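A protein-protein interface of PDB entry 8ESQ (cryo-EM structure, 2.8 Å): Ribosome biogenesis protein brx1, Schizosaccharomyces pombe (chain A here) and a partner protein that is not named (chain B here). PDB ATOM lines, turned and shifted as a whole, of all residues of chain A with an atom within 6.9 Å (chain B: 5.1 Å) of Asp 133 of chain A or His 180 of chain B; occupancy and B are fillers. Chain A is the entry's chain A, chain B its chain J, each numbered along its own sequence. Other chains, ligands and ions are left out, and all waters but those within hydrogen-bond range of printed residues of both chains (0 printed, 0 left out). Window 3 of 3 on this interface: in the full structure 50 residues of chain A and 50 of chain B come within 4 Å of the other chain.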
ATOM      1  N   HIS A  59       9.301  18.949 -37.345  1.00  0.00           N
ATOM      2  CA  HIS A  59      10.058  18.932 -36.100  1.00  0.00           C
ATOM      3  C   HIS A  59      11.530  19.224 -36.353  1.00  0.00           C
ATOM      4  O   HIS A  59      12.141  20.023 -35.636  1.00  0.00           O
ATOM      5  CB  HIS A  59       9.891  17.587 -35.395  1.00  0.00           C
ATOM      6  CG  HIS A  59       8.610  17.458 -34.633  1.00  0.00           C
ATOM      7  ND1 HIS A  59       7.517  16.778 -35.123  1.00  0.00           N
ATOM      8  CD2 HIS A  59       8.248  17.922 -33.414  1.00  0.00           C
ATOM      9  CE1 HIS A  59       6.537  16.828 -34.240  1.00  0.00           C
ATOM     10  NE2 HIS A  59       6.954  17.517 -33.193  1.00  0.00           N
ATOM     11  N   ASP A  63      13.529  22.156 -34.716  1.00  0.00           N
ATOM     12  CA  ASP A  63      14.721  21.805 -33.954  1.00  0.00           C
ATOM     13  C   ASP A  63      15.956  22.517 -34.492  1.00  0.00           C
ATOM     14  O   ASP A  63      16.787  22.999 -33.717  1.00  0.00           O
ATOM     15  CB  ASP A  63      14.908  20.290 -33.979  1.00  0.00           C
ATOM     16  CG  ASP A  63      13.804  19.560 -33.240  1.00  0.00           C
ATOM     17  OD1 ASP A  63      12.723  20.154 -33.046  1.00  0.00           O
ATOM     18  OD2 ASP A  63      13.988  18.370 -32.911  1.00  0.00           O
ATOM     19  N   HIS A 130      15.872  12.002 -36.254  1.00  0.00           N
ATOM     20  CA  HIS A 130      15.681  11.893 -34.813  1.00  0.00           C
ATOM     21  C   HIS A 130      15.544  13.292 -34.232  1.00  0.00           C
ATOM     22  O   HIS A 130      16.388  14.156 -34.489  1.00  0.00           O
ATOM     23  CB  HIS A 130      16.841  11.135 -34.159  1.00  0.00           C
ATOM     24  CG  HIS A 130      17.026   9.745 -34.686  1.00  0.00           C
ATOM     25  ND1 HIS A 130      16.185   8.706 -34.351  1.00  0.00           N
ATOM     26  CD2 HIS A 130      17.948   9.225 -35.530  1.00  0.00           C
ATOM     27  CE1 HIS A 130      16.584   7.604 -34.960  1.00  0.00           C
ATOM     28  NE2 HIS A 130      17.652   7.892 -35.683  1.00  0.00           N
ATOM     29  N   THR A 131      14.486  13.515 -33.453  1.00  0.00           N
ATOM     30  CA  THR A 131      14.128  14.842 -32.981  1.00  0.00           C
ATOM     31  C   THR A 131      14.411  14.987 -31.486  1.00  0.00           C
ATOM     32  O   THR A 131      14.892  14.067 -30.822  1.00  0.00           O
ATOM     33  CB  THR A 131      12.657  15.131 -33.289  1.00  0.00           C
ATOM     34  OG1 THR A 131      11.832  14.126 -32.684  1.00  0.00           O
ATOM     35  CG2 THR A 131      12.431  15.123 -34.788  1.00  0.00           C
ATOM     36  N   MET A 132      14.099  16.174 -30.952  1.00  0.00           N
ATOM     37  CA  MET A 132      14.341  16.442 -29.536  1.00  0.00           C
ATOM     38  C   MET A 132      13.522  15.522 -28.647  1.00  0.00           C
ATOM     39  O   MET A 132      14.037  14.975 -27.665  1.00  0.00           O
ATOM     40  CB  MET A 132      14.017  17.900 -29.205  1.00  0.00           C
ATOM     41  CG  MET A 132      14.708  19.014 -30.010  1.00  0.00           C
ATOM     42  SD  MET A 132      16.490  18.975 -30.369  1.00  0.00           S
ATOM     43  CE  MET A 132      16.698  17.687 -31.593  1.00  0.00           C
ATOM     44  N   ASP A 133      12.249  15.327 -28.983  1.00  0.00           N
ATOM     45  CA  ASP A 133      11.337  14.573 -28.136  1.00  0.00           C
ATOM     46  C   ASP A 133      11.634  13.080 -28.122  1.00  0.00           C
ATOM     47  O   ASP A 133      10.988  12.348 -27.363  1.00  0.00           O
ATOM     48  CB  ASP A 133       9.896  14.818 -28.585  1.00  0.00           C
ATOM     49  CG  ASP A 133       8.903  14.676 -27.453  1.00  0.00           C
ATOM     50  OD1 ASP A 133       9.259  15.026 -26.308  1.00  0.00           O
ATOM     51  OD2 ASP A 133       7.767  14.222 -27.705  1.00  0.00           O
ATOM     52  N   GLU A 134      12.575  12.607 -28.937  1.00  0.00           N
ATOM     53  CA  GLU A 134      12.922  11.194 -28.928  1.00  0.00           C
ATOM     54  C   GLU A 134      13.521  10.804 -27.581  1.00  0.00           C
ATOM     55  O   GLU A 134      14.223  11.591 -26.942  1.00  0.00           O
ATOM     56  CB  GLU A 134      13.889  10.872 -30.064  1.00  0.00           C
ATOM     57  CG  GLU A 134      13.182  10.562 -31.375  1.00  0.00           C
ATOM     58  CD  GLU A 134      14.037   9.763 -32.334  1.00  0.00           C
ATOM     59  OE1 GLU A 134      15.141   9.336 -31.937  1.00  0.00           O
ATOM     60  OE2 GLU A 134      13.603   9.560 -33.487  1.00  0.00           O
ATOM     61  N   LEU A 135      13.227   9.575 -27.155  1.00  0.00           N
ATOM     62  CA  LEU A 135      13.473   9.179 -25.771  1.00  0.00           C
ATOM     63  C   LEU A 135      14.962   9.140 -25.444  1.00  0.00           C
ATOM     64  O   LEU A 135      15.376   9.559 -24.357  1.00  0.00           O
ATOM     65  CB  LEU A 135      12.837   7.815 -25.504  1.00  0.00           C
ATOM     66  CG  LEU A 135      11.376   7.631 -25.928  1.00  0.00           C
ATOM     67  CD1 LEU A 135      10.900   6.221 -25.605  1.00  0.00           C
ATOM     68  CD2 LEU A 135      10.459   8.675 -25.312  1.00  0.00           C
ATOM     69  N   ASN A 136      15.779   8.632 -26.370  1.00  0.00           N
ATOM     70  CA  ASN A 136      17.157   8.277 -26.041  1.00  0.00           C
ATOM     71  C   ASN A 136      17.989   9.494 -25.650  1.00  0.00           C
ATOM     72  O   ASN A 136      18.726   9.457 -24.658  1.00  0.00           O
ATOM     73  CB  ASN A 136      17.802   7.553 -27.222  1.00  0.00           C
ATOM     74  CG  ASN A 136      16.849   6.597 -27.911  1.00  0.00           C
ATOM     75  OD1 ASN A 136      15.702   6.943 -28.197  1.00  0.00           O
ATOM     76  ND2 ASN A 136      17.322   5.387 -28.186  1.00  0.00           N
ATOM     77  N   MET A 137      17.886  10.579 -26.412  1.00  0.00           N
ATOM     78  CA  MET A 137      18.767  11.724 -26.231  1.00  0.00           C
ATOM     79  C   MET A 137      18.444  12.475 -24.945  1.00  0.00           C
ATOM     80  O   MET A 137      17.272  12.670 -24.606  1.00  0.00           O
ATOM     81  CB  MET A 137      18.666  12.660 -27.433  1.00  0.00           C
ATOM     82  CG  MET A 137      18.148  11.988 -28.695  1.00  0.00           C
ATOM     83  SD  MET A 137      19.054  10.473 -29.072  1.00  0.00           S
ATOM     84  CE  MET A 137      17.898   9.633 -30.150  1.00  0.00           C
ATOM     85  N   GLY A 139      20.799  15.307 -24.126  1.00  0.00           N
ATOM     86  CA  GLY A 139      21.675  16.461 -24.153  1.00  0.00           C
ATOM     87  C   GLY A 139      20.930  17.763 -23.928  1.00  0.00           C
ATOM     88  O   GLY A 139      19.714  17.858 -24.093  1.00  0.00           O
ATOM     89  N   LYS B 176      16.085  22.511 -25.122  1.00  0.00           N
ATOM     90  CA  LYS B 176      15.071  21.517 -24.808  1.00  0.00           C
ATOM     91  C   LYS B 176      14.134  22.073 -23.749  1.00  0.00           C
ATOM     92  O   LYS B 176      14.587  22.624 -22.740  1.00  0.00           O
ATOM     93  CB  LYS B 176      15.716  20.223 -24.318  1.00  0.00           C
ATOM     94  CG  LYS B 176      16.710  19.621 -25.283  1.00  0.00           C
ATOM     95  CD  LYS B 176      15.989  18.840 -26.358  1.00  0.00           C
ATOM     96  CE  LYS B 176      16.927  17.873 -27.047  1.00  0.00           C
ATOM     97  NZ  LYS B 176      17.339  16.746 -26.165  1.00  0.00           N
ATOM     98  N   SER B 177      12.834  21.936 -23.987  1.00  0.00           N
ATOM     99  CA  SER B 177      11.846  22.399 -23.027  1.00  0.00           C
ATOM    100  C   SER B 177      11.957  21.607 -21.733  1.00  0.00           C
ATOM    101  O   SER B 177      12.153  20.389 -21.746  1.00  0.00           O
ATOM    102  CB  SER B 177      10.439  22.263 -23.604  1.00  0.00           C
ATOM    103  OG  SER B 177       9.464  22.285 -22.577  1.00  0.00           O
ATOM    104  N   ASP B 178      11.829  22.311 -20.606  1.00  0.00           N
ATOM    105  CA  ASP B 178      11.916  21.649 -19.311  1.00  0.00           C
ATOM    106  C   ASP B 178      10.793  20.637 -19.128  1.00  0.00           C
ATOM    107  O   ASP B 178      10.957  19.653 -18.397  1.00  0.00           O
ATOM    108  CB  ASP B 178      11.884  22.690 -18.191  1.00  0.00           C
ATOM    109  CG  ASP B 178      13.252  22.949 -17.595  1.00  0.00           C
ATOM    110  OD1 ASP B 178      14.259  22.540 -18.209  1.00  0.00           O
ATOM    111  OD2 ASP B 178      13.323  23.570 -16.514  1.00  0.00           O
ATOM    112  N   ASP B 179       9.654  20.856 -19.791  1.00  0.00           N
ATOM    113  CA  ASP B 179       8.505  19.972 -19.624  1.00  0.00           C
ATOM    114  C   ASP B 179       8.824  18.581 -20.161  1.00  0.00           C
ATOM    115  O   ASP B 179       8.607  17.575 -19.476  1.00  0.00           O
ATOM    116  CB  ASP B 179       7.279  20.606 -20.308  1.00  0.00           C
ATOM    117  CG  ASP B 179       6.100  19.638 -20.540  1.00  0.00           C
ATOM    118  OD1 ASP B 179       6.259  18.412 -20.697  1.00  0.00           O
ATOM    119  OD2 ASP B 179       4.957  20.141 -20.563  1.00  0.00           O
ATOM    120  N   HIS B 180       9.332  18.501 -21.395  1.00  0.00           N
ATOM    121  CA  HIS B 180       9.711  17.199 -21.928  1.00  0.00           C
ATOM    122  C   HIS B 180      11.029  16.712 -21.345  1.00  0.00           C
ATOM    123  O   HIS B 180      11.307  15.510 -21.395  1.00  0.00           O
ATOM    124  CB  HIS B 180       9.794  17.237 -23.455  1.00  0.00           C
ATOM    125  CG  HIS B 180      11.112  17.712 -23.983  1.00  0.00           C
ATOM    126  ND1 HIS B 180      12.168  16.858 -24.219  1.00  0.00           N
ATOM    127  CD2 HIS B 180      11.541  18.946 -24.336  1.00  0.00           C
ATOM    128  CE1 HIS B 180      13.193  17.547 -24.684  1.00  0.00           C
ATOM    129  NE2 HIS B 180      12.839  18.816 -24.766  1.00  0.00           N
ATOM    130  N   MET B 181      11.845  17.614 -20.794  1.00  0.00           N
ATOM    131  CA  MET B 181      12.988  17.170 -20.006  1.00  0.00           C
ATOM    132  C   MET B 181      12.536  16.366 -18.802  1.00  0.00           C
ATOM    133  O   MET B 181      13.170  15.372 -18.433  1.00  0.00           O
ATOM    134  CB  MET B 181      13.835  18.357 -19.560  1.00  0.00           C
ATOM    135  CG  MET B 181      14.733  18.868 -20.638  1.00  0.00           C
ATOM    136  SD  MET B 181      16.346  18.109 -20.420  1.00  0.00           S
ATOM    137  CE  MET B 181      17.313  19.157 -21.474  1.00  0.00           C
ATOM    138  N   GLU B 182      11.442  16.787 -18.171  1.00  0.00           N
ATOM    139  CA  GLU B 182      10.902  16.001 -17.074  1.00  0.00           C
ATOM    140  C   GLU B 182      10.392  14.655 -17.578  1.00  0.00           C
ATOM    141  O   GLU B 182      10.497  13.646 -16.870  1.00  0.00           O
ATOM    142  CB  GLU B 182       9.805  16.788 -16.357  1.00  0.00           C
ATOM    143  CG  GLU B 182       9.274  16.112 -15.110  1.00  0.00           C
ATOM    144  CD  GLU B 182      10.365  15.410 -14.319  1.00  0.00           C
ATOM    145  OE1 GLU B 182      11.309  16.092 -13.868  1.00  0.00           O
ATOM    146  OE2 GLU B 182      10.277  14.177 -14.147  1.00  0.00           O
ATOM    147  N   LYS B 183       9.855  14.610 -18.806  1.00  0.00           N
ATOM    148  CA  LYS B 183       9.487  13.324 -19.396  1.00  0.00           C
ATOM    149  C   LYS B 183      10.712  12.450 -19.621  1.00  0.00           C
ATOM    150  O   LYS B 183      10.702  11.258 -19.290  1.00  0.00           O
ATOM    151  CB  LYS B 183       8.745  13.500 -20.721  1.00  0.00           C
ATOM    152  CG  LYS B 183       7.450  14.284 -20.691  1.00  0.00           C
ATOM    153  CD  LYS B 183       7.039  14.586 -22.128  1.00  0.00           C
ATOM    154  CE  LYS B 183       6.040  15.712 -22.248  1.00  0.00           C
ATOM    155  NZ  LYS B 183       6.112  16.312 -23.608  1.00  0.00           N
ATOM    156  N   VAL B 184      11.773  13.024 -20.192  1.00  0.00           N
ATOM    157  CA  VAL B 184      13.021  12.291 -20.369  1.00  0.00           C
ATOM    158  C   VAL B 184      13.544  11.819 -19.021  1.00  0.00           C
ATOM    159  O   VAL B 184      14.124  10.733 -18.903  1.00  0.00           O
ATOM    160  CB  VAL B 184      14.045  13.170 -21.108  1.00  0.00           C
ATOM    161  CG1 VAL B 184      15.466  12.787 -20.725  1.00  0.00           C
ATOM    162  CG2 VAL B 184      13.844  13.068 -22.613  1.00  0.00           C
ATOM    163  N   ARG B 185      13.332  12.623 -17.978  1.00  0.00           N
ATOM    164  CA  ARG B 185      13.719  12.205 -16.636  1.00  0.00           C
ATOM    165  C   ARG B 185      12.886  11.018 -16.158  1.00  0.00           C
ATOM    166  O   ARG B 185      13.438  10.056 -15.611  1.00  0.00           O
ATOM    167  CB  ARG B 185      13.619  13.386 -15.672  1.00  0.00           C
ATOM    168  CG  ARG B 185      14.915  13.650 -14.925  1.00  0.00           C
ATOM    169  CD  ARG B 185      16.021  14.080 -15.881  1.00  0.00           C
ATOM    170  NE  ARG B 185      17.036  14.881 -15.209  1.00  0.00           N
ATOM    171  CZ  ARG B 185      18.105  15.395 -15.802  1.00  0.00           C
ATOM    172  NH1 ARG B 185      18.341  15.205 -17.090  1.00  0.00           N
ATOM    173  NH2 ARG B 185      18.962  16.113 -15.083  1.00  0.00           N
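The side-chain amino group of Lys 176 of chain B sits at hydrogen-bond distance from the backbone carbonyl oxygen of Gly 139 of chain A, at 3.3 Å.
Met 132 of chain A touches Lys 176 of chain B.
Asp 133 of chain A touches His 180 of chain B.
Val 184 of chain B touches Met 137 of chain A.
Gly 139 of chain A touches Met 181 of chain B (O to CE, 3.8 Å).
N of Met 132 of chain A is in hydrogen-bond range of OD2 of Asp 63 of chain A (2.9 Å).
N of Ser 177 of chain B lies within hydrogen-bond range of NE2 of His 180 of chain B.
Of the 10 printed residues of chain B, 4 touch a printed residue of chain A.
Hydrophobic or aromatic side chains of chain B within 4 Å of the printed part of chain A: His 180, Met 181 and Val 184.
Along chain B the printed residues that touch a printed residue of chain A span positions 176 to 184.
Among the printed residues, no Asp or Glu carboxylate lies within 4 Å of a Lys or Arg side-chain nitrogen of the other chain.
Of chain A, only Asp 133 comes within 4 Å of His 180 of chain B.
Printed residues of chain B within 4 Å of Met 137 of chain A: Val 184.
Printed residues of chain A within 4 Å of Met 181 of chain B: Gly 139 (3.8 Å).
Printed residues of chain A within 4 Å of Val 184 of chain B: Met 137 (3.99 Å).
Of the printed residues of chain B, Gly 139 of chain A touches Lys 176 (3.3 Å) and Met 181 (3.8 Å).
The nearest residue of chain A that does not touch His 180 of chain B is Met 132 of chain A (4.03 Å).
The nearest printed residue of chain B that does not touch Met 137 of chain A is Lys 176 of chain B (4.4 Å).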
